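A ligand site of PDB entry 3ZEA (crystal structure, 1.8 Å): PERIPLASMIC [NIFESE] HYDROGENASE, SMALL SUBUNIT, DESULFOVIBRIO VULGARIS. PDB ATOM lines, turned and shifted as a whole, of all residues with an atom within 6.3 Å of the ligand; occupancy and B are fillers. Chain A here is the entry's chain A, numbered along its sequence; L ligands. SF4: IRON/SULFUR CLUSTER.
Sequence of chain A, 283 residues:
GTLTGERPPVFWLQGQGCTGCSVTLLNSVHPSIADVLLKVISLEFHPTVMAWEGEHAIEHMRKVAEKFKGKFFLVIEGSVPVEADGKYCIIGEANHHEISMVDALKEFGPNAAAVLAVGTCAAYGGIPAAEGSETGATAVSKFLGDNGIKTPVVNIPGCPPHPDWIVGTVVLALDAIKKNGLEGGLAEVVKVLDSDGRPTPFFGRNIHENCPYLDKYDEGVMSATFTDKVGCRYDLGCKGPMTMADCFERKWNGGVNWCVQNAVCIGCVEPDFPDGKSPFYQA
The guanidinium group (NE) of Arg 233 lies within hydrogen-bond range of the backbone carbonyl oxygen (O) of Val 260, at 2.8 Å. The side-chain sulfur (SG) of Cys 232 sits close to the side-chain sulfur (SD) of Met 222 (3.7 Å). The side-chain sulfur (SG) of Cys 238 sits close to the backbone NH (N) of Gly 240 (3.5 Å). N of Cys 238 lies within hydrogen-bond range of O of Arg 233 (3.2 Å). N of Tyr 234 sits close to SG of Cys 232, 3.3 Å away. The side-chain sulfur (SG) of Cys 238 lies close to the backbone NH (N) of Cys 265 (3.8 Å). O of Gly 240 lies within hydrogen-bond range of N of His 208 (3.4 Å). NH1 of Arg 233 is in hydrogen-bond range of O of Gly 231.
FE2 of the ligand is bound by ND1 of His 208 (2.1 Å). S1 of the ligand sits close to N of Leu 214 (3.5 Å). SG of Cys 238 is bound to FE1 of the ligand (2.3 Å). N of Arg 233 lies close to S2 of the ligand, 3.3 Å away. SG of Cys 232 binds FE3 of the ligand (2.3 Å). The side-chain sulfur (SG) of Cys 211 binds an iron atom (FE4) of the ligand (2.3 Å).
O of Tyr 213 lies close to S1 of the ligand (3.7 Å). Merely in contact with the ligand: Ile 207, Tyr 217, Tyr 234, Gly 240, Pro 241 and Val 260. 13 residues have an atom within 4 Å of the ligand: Ile 207, His 208, Cys 211, Tyr 213, Leu 214, Tyr 217, Cys 232, Arg 233, Tyr 234, Cys 238, Gly 240, Pro 241 and Val 260. The nearest printed residue that does not touch the ligand is Lys 239 (5.3 Å).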
ATOM      1  N   ILE A 207       5.085  27.318  20.216  1.00  0.00           N
ATOM      2  CA  ILE A 207       5.358  26.057  20.900  1.00  0.00           C
ATOM      3  C   ILE A 207       4.834  24.860  20.096  1.00  0.00           C
ATOM      4  O   ILE A 207       5.569  23.913  19.821  1.00  0.00           O
ATOM      5  CB  ILE A 207       4.690  26.049  22.293  1.00  0.00           C
ATOM      6  CG1 ILE A 207       5.360  27.068  23.225  1.00  0.00           C
ATOM      7  CG2 ILE A 207       4.754  24.660  22.891  1.00  0.00           C
ATOM      8  CD1 ILE A 207       6.594  26.599  23.886  1.00  0.00           C
ATOM      9  N   HIS A 208       3.563  24.895  19.722  1.00  0.00           N
ATOM     10  CA  HIS A 208       2.890  23.753  19.111  1.00  0.00           C
ATOM     11  C   HIS A 208       3.508  23.348  17.771  1.00  0.00           C
ATOM     12  O   HIS A 208       3.766  22.164  17.517  1.00  0.00           O
ATOM     13  CB  HIS A 208       1.426  24.154  18.940  1.00  0.00           C
ATOM     14  CG  HIS A 208       0.594  23.175  18.174  1.00  0.00           C
ATOM     15  ND1 HIS A 208       0.125  21.998  18.720  1.00  0.00           N
ATOM     16  CD2 HIS A 208       0.099  23.228  16.912  1.00  0.00           C
ATOM     17  CE1 HIS A 208      -0.603  21.356  17.818  1.00  0.00           C
ATOM     18  NE2 HIS A 208      -0.636  22.088  16.713  1.00  0.00           N
ATOM     19  N   GLU A 209       3.754  24.314  16.890  1.00  0.00           N
ATOM     20  CA  GLU A 209       4.237  23.971  15.549  1.00  0.00           C
ATOM     21  C   GLU A 209       5.658  23.415  15.618  1.00  0.00           C
ATOM     22  O   GLU A 209       6.143  22.805  14.661  1.00  0.00           O
ATOM     23  CB  GLU A 209       4.153  25.184  14.613  1.00  0.00           C
ATOM     24  CG  GLU A 209       2.677  25.645  14.310  1.00  0.00           C
ATOM     25  CD  GLU A 209       1.811  24.607  13.596  1.00  0.00           C
ATOM     26  OE1 GLU A 209       2.342  23.689  12.931  1.00  0.00           O
ATOM     27  OE2 GLU A 209       0.563  24.707  13.684  1.00  0.00           O
ATOM     28  N   CYS A 211       6.478  21.406  18.348  1.00  0.00           N
ATOM     29  CA  CYS A 211       6.373  20.461  19.435  1.00  0.00           C
ATOM     30  C   CYS A 211       6.691  19.059  18.991  1.00  0.00           C
ATOM     31  O   CYS A 211       6.253  18.632  17.918  1.00  0.00           O
ATOM     32  CB  CYS A 211       4.955  20.452  19.980  1.00  0.00           C
ATOM     33  SG  CYS A 211       4.731  19.347  21.427  1.00  0.00           S
ATOM     34  N   PRO A 212       7.429  18.310  19.817  1.00  0.00           N
ATOM     35  CA  PRO A 212       7.751  16.916  19.481  1.00  0.00           C
ATOM     36  C   PRO A 212       6.508  16.004  19.390  1.00  0.00           C
ATOM     37  O   PRO A 212       6.586  14.917  18.813  1.00  0.00           O
ATOM     38  CB  PRO A 212       8.657  16.479  20.635  1.00  0.00           C
ATOM     39  CG  PRO A 212       8.394  17.429  21.727  1.00  0.00           C
ATOM     40  CD  PRO A 212       8.109  18.734  21.054  1.00  0.00           C
ATOM     41  N   TYR A 213       5.381  16.437  19.940  1.00  0.00           N
ATOM     42  CA  TYR A 213       4.187  15.615  19.918  1.00  0.00           C
ATOM     43  C   TYR A 213       3.223  16.014  18.815  1.00  0.00           C
ATOM     44  O   TYR A 213       2.126  15.499  18.727  1.00  0.00           O
ATOM     45  CB  TYR A 213       3.491  15.661  21.282  1.00  0.00           C
ATOM     46  CG  TYR A 213       4.429  15.232  22.365  1.00  0.00           C
ATOM     47  CD1 TYR A 213       4.870  13.916  22.430  1.00  0.00           C
ATOM     48  CD2 TYR A 213       4.920  16.137  23.295  1.00  0.00           C
ATOM     49  CE1 TYR A 213       5.757  13.516  23.396  1.00  0.00           C
ATOM     50  CE2 TYR A 213       5.815  15.732  24.264  1.00  0.00           C
ATOM     51  CZ  TYR A 213       6.227  14.420  24.315  1.00  0.00           C
ATOM     52  OH  TYR A 213       7.108  14.009  25.275  1.00  0.00           O
ATOM     53  N   LEU A 214       3.646  16.938  17.960  1.00  0.00           N
ATOM     54  CA  LEU A 214       2.783  17.399  16.874  1.00  0.00           C
ATOM     55  C   LEU A 214       2.248  16.271  15.989  1.00  0.00           C
ATOM     56  O   LEU A 214       1.114  16.315  15.502  1.00  0.00           O
ATOM     57  CB  LEU A 214       3.527  18.444  16.031  1.00  0.00           C
ATOM     58  CG  LEU A 214       2.736  19.209  14.971  1.00  0.00           C
ATOM     59  CD1 LEU A 214       1.577  19.981  15.549  1.00  0.00           C
ATOM     60  CD2 LEU A 214       3.668  20.143  14.234  1.00  0.00           C
ATOM     61  N   ASP A 215       3.076  15.258  15.716  1.00  0.00           N
ATOM     62  CA  ASP A 215       2.627  14.146  14.870  1.00  0.00           C
ATOM     63  C   ASP A 215       1.445  13.427  15.514  1.00  0.00           C
ATOM     64  O   ASP A 215       0.530  12.992  14.816  1.00  0.00           O
ATOM     65  CB  ASP A 215       3.781  13.189  14.543  1.00  0.00           C
ATOM     66  CG  ASP A 215       4.496  12.649  15.779  1.00  0.00           C
ATOM     67  OD1 ASP A 215       4.353  13.242  16.877  1.00  0.00           O
ATOM     68  OD2 ASP A 215       5.209  11.630  15.665  1.00  0.00           O
ATOM     69  N   LYS A 216       1.449  13.327  16.845  1.00  0.00           N
ATOM     70  CA  LYS A 216       0.345  12.705  17.564  1.00  0.00           C
ATOM     71  C   LYS A 216      -0.914  13.581  17.514  1.00  0.00           C
ATOM     72  O   LYS A 216      -2.017  13.079  17.296  1.00  0.00           O
ATOM     73  CB  LYS A 216       0.725  12.402  19.008  1.00  0.00           C
ATOM     74  CG  LYS A 216       1.945  11.515  19.141  1.00  0.00           C
ATOM     75  CD  LYS A 216       1.622  10.079  18.755  1.00  0.00           C
ATOM     76  CE  LYS A 216       2.829   9.187  18.913  1.00  0.00           C
ATOM     77  NZ  LYS A 216       2.601   7.856  18.330  1.00  0.00           N
ATOM     78  N   TYR A 217      -0.739  14.882  17.708  1.00  0.00           N
ATOM     79  CA  TYR A 217      -1.837  15.812  17.533  1.00  0.00           C
ATOM     80  C   TYR A 217      -2.502  15.583  16.174  1.00  0.00           C
ATOM     81  O   TYR A 217      -3.715  15.450  16.080  1.00  0.00           O
ATOM     82  CB  TYR A 217      -1.310  17.237  17.626  1.00  0.00           C
ATOM     83  CG  TYR A 217      -2.314  18.313  17.368  1.00  0.00           C
ATOM     84  CD1 TYR A 217      -3.118  18.808  18.388  1.00  0.00           C
ATOM     85  CD2 TYR A 217      -2.448  18.870  16.103  1.00  0.00           C
ATOM     86  CE1 TYR A 217      -4.030  19.826  18.150  1.00  0.00           C
ATOM     87  CE2 TYR A 217      -3.373  19.882  15.856  1.00  0.00           C
ATOM     88  CZ  TYR A 217      -4.160  20.354  16.889  1.00  0.00           C
ATOM     89  OH  TYR A 217      -5.070  21.365  16.666  1.00  0.00           O
ATOM     90  N   MET A 222      -4.342  11.244  21.650  1.00  0.00           N
ATOM     91  CA  MET A 222      -4.301  12.168  22.797  1.00  0.00           C
ATOM     92  C   MET A 222      -4.179  11.406  24.087  1.00  0.00           C
ATOM     93  O   MET A 222      -4.913  10.455  24.332  1.00  0.00           O
ATOM     94  CB  MET A 222      -5.632  12.908  22.860  1.00  0.00           C
ATOM     95  CG  MET A 222      -5.945  13.677  21.651  1.00  0.00           C
ATOM     96  SD  MET A 222      -4.847  15.073  21.660  1.00  0.00           S
ATOM     97  CE  MET A 222      -5.079  15.677  19.998  1.00  0.00           C
ATOM     98  N   GLY A 231       1.120  10.276  23.945  1.00  0.00           N
ATOM     99  CA  GLY A 231       0.119  11.059  23.241  1.00  0.00           C
ATOM    100  C   GLY A 231       0.288  12.568  23.327  1.00  0.00           C
ATOM    101  O   GLY A 231       1.042  13.073  24.142  1.00  0.00           O
ATOM    102  N   CYS A 232      -0.405  13.282  22.453  1.00  0.00           N
ATOM    103  CA  CYS A 232      -0.458  14.735  22.551  1.00  0.00           C
ATOM    104  C   CYS A 232      -1.256  15.131  23.813  1.00  0.00           C
ATOM    105  O   CYS A 232      -2.157  14.382  24.231  1.00  0.00           O
ATOM    106  CB  CYS A 232      -1.083  15.291  21.276  1.00  0.00           C
ATOM    107  SG  CYS A 232      -1.713  16.996  21.379  1.00  0.00           S
ATOM    108  N   ARG A 233      -0.899  16.287  24.410  1.00  0.00           N
ATOM    109  CA  ARG A 233      -1.492  16.758  25.672  1.00  0.00           C
ATOM    110  C   ARG A 233      -2.696  17.682  25.498  1.00  0.00           C
ATOM    111  O   ARG A 233      -3.186  18.278  26.474  1.00  0.00           O
ATOM    112  CB  ARG A 233      -0.439  17.514  26.490  1.00  0.00           C
ATOM    113  CG  ARG A 233       0.639  16.679  27.166  1.00  0.00           C
ATOM    114  CD  ARG A 233       1.587  15.945  26.203  1.00  0.00           C
ATOM    115  NE  ARG A 233       2.808  15.591  26.906  1.00  0.00           N
ATOM    116  CZ  ARG A 233       3.602  14.564  26.629  1.00  0.00           C
ATOM    117  NH1 ARG A 233       3.344  13.709  25.611  1.00  0.00           N
ATOM    118  NH2 ARG A 233       4.670  14.376  27.368  1.00  0.00           N
ATOM    119  N   TYR A 234      -3.171  17.820  24.271  1.00  0.00           N
ATOM    120  CA  TYR A 234      -4.233  18.763  23.956  1.00  0.00           C
ATOM    121  C   TYR A 234      -5.509  18.545  24.790  1.00  0.00           C
ATOM    122  O   TYR A 234      -6.088  19.511  25.295  1.00  0.00           O
ATOM    123  CB  TYR A 234      -4.546  18.716  22.468  1.00  0.00           C
ATOM    124  CG  TYR A 234      -5.620  19.674  22.077  1.00  0.00           C
ATOM    125  CD1 TYR A 234      -5.329  21.012  21.861  1.00  0.00           C
ATOM    126  CD2 TYR A 234      -6.928  19.255  21.980  1.00  0.00           C
ATOM    127  CE1 TYR A 234      -6.321  21.896  21.521  1.00  0.00           C
ATOM    128  CE2 TYR A 234      -7.933  20.120  21.639  1.00  0.00           C
ATOM    129  CZ  TYR A 234      -7.619  21.440  21.398  1.00  0.00           C
ATOM    130  OH  TYR A 234      -8.630  22.303  21.069  1.00  0.00           O
ATOM    131  N   CYS A 238      -3.415  21.354  27.144  1.00  0.00           N
ATOM    132  CA  CYS A 238      -2.211  22.031  26.601  1.00  0.00           C
ATOM    133  C   CYS A 238      -2.577  23.248  25.746  1.00  0.00           C
ATOM    134  O   CYS A 238      -3.404  23.149  24.823  1.00  0.00           O
ATOM    135  CB  CYS A 238      -1.378  21.044  25.754  1.00  0.00           C
ATOM    136  SG  CYS A 238       0.201  21.757  25.258  1.00  0.00           S
ATOM    137  N   LYS A 239      -1.958  24.392  26.063  1.00  0.00           N
ATOM    138  CA  LYS A 239      -2.210  25.643  25.340  1.00  0.00           C
ATOM    139  C   LYS A 239      -1.053  25.980  24.363  1.00  0.00           C
ATOM    140  O   LYS A 239      -0.954  27.108  23.868  1.00  0.00           O
ATOM    141  CB  LYS A 239      -2.423  26.801  26.339  1.00  0.00           C
ATOM    142  CG  LYS A 239      -3.610  26.598  27.302  1.00  0.00           C
ATOM    143  CD  LYS A 239      -4.892  26.185  26.574  1.00  0.00           C
ATOM    144  CE  LYS A 239      -6.109  26.165  27.511  1.00  0.00           C
ATOM    145  NZ  LYS A 239      -5.831  25.380  28.715  1.00  0.00           N
ATOM    146  N   GLY A 240      -0.202  25.004  24.062  1.00  0.00           N
ATOM    147  CA  GLY A 240       0.839  25.173  23.056  1.00  0.00           C
ATOM    148  C   GLY A 240       0.397  25.858  21.764  1.00  0.00           C
ATOM    149  O   GLY A 240       1.127  26.699  21.227  1.00  0.00           O
ATOM    150  N   PRO A 241      -0.791  25.494  21.214  1.00  0.00           N
ATOM    151  CA  PRO A 241      -1.169  26.131  19.937  1.00  0.00           C
ATOM    152  C   PRO A 241      -1.279  27.630  20.000  1.00  0.00           C
ATOM    153  O   PRO A 241      -1.069  28.315  18.970  1.00  0.00           O
ATOM    154  CB  PRO A 241      -2.552  25.492  19.636  1.00  0.00           C
ATOM    155  CG  PRO A 241      -2.496  24.180  20.263  1.00  0.00           C
ATOM    156  CD  PRO A 241      -1.704  24.396  21.563  1.00  0.00           C
ATOM    157  N   TRP A 258      10.528  20.320  30.666  1.00  0.00           N
ATOM    158  CA  TRP A 258       9.725  21.482  30.335  1.00  0.00           C
ATOM    159  C   TRP A 258       8.254  21.126  30.483  1.00  0.00           C
ATOM    160  O   TRP A 258       7.906  19.958  30.656  1.00  0.00           O
ATOM    161  CB  TRP A 258      10.039  22.008  28.939  1.00  0.00           C
ATOM    162  CG  TRP A 258       9.679  21.124  27.765  1.00  0.00           C
ATOM    163  CD1 TRP A 258      10.130  19.868  27.507  1.00  0.00           C
ATOM    164  CD2 TRP A 258       8.841  21.480  26.654  1.00  0.00           C
ATOM    165  NE1 TRP A 258       9.621  19.399  26.309  1.00  0.00           N
ATOM    166  CE2 TRP A 258       8.844  20.389  25.762  1.00  0.00           C
ATOM    167  CE3 TRP A 258       8.111  22.625  26.333  1.00  0.00           C
ATOM    168  CZ2 TRP A 258       8.115  20.399  24.572  1.00  0.00           C
ATOM    169  CZ3 TRP A 258       7.376  22.624  25.138  1.00  0.00           C
ATOM    170  CH2 TRP A 258       7.388  21.529  24.282  1.00  0.00           C
ATOM    171  N   VAL A 260       5.459  20.887  28.687  1.00  0.00           N
ATOM    172  CA  VAL A 260       4.716  19.967  27.826  1.00  0.00           C
ATOM    173  C   VAL A 260       5.145  18.521  28.092  1.00  0.00           C
ATOM    174  O   VAL A 260       4.302  17.628  28.090  1.00  0.00           O
ATOM    175  CB  VAL A 260       4.895  20.349  26.355  1.00  0.00           C
ATOM    176  CG1 VAL A 260       4.265  19.294  25.419  1.00  0.00           C
ATOM    177  CG2 VAL A 260       4.291  21.711  26.095  1.00  0.00           C
ATOM    178  N   CYS A 265       1.375  22.798  28.718  1.00  0.00           N
ATOM    179  CA  CYS A 265       1.646  24.237  28.641  1.00  0.00           C
ATOM    180  C   CYS A 265       0.396  25.002  29.074  1.00  0.00           C
ATOM    181  O   CYS A 265      -0.727  24.665  28.637  1.00  0.00           O
ATOM    182  CB  CYS A 265       2.047  24.618  27.219  1.00  0.00           C
ATOM    183  SG  CYS A 265       2.294  26.424  26.898  1.00  0.00           S
HETATM  184 FE1  SF4 L   1       0.558  20.695  23.237  1.00  0.00          FE
HETATM  185 FE2  SF4 L   1       0.487  20.986  20.503  1.00  0.00          FE
HETATM  186 FE3  SF4 L   1      -0.060  18.570  21.556  1.00  0.00          FE
HETATM  187 FE4  SF4 L   1       2.458  19.601  21.649  1.00  0.00          FE
HETATM  188  S1  SF4 L   1       1.334  18.934  19.762  1.00  0.00           S
HETATM  189  S2  SF4 L   1       1.358  18.525  23.353  1.00  0.00           S
HETATM  190  S3  SF4 L   1       2.052  21.884  21.945  1.00  0.00           S
HETATM  191  S4  SF4 L   1      -1.307  20.492  21.871  1.00  0.00           S
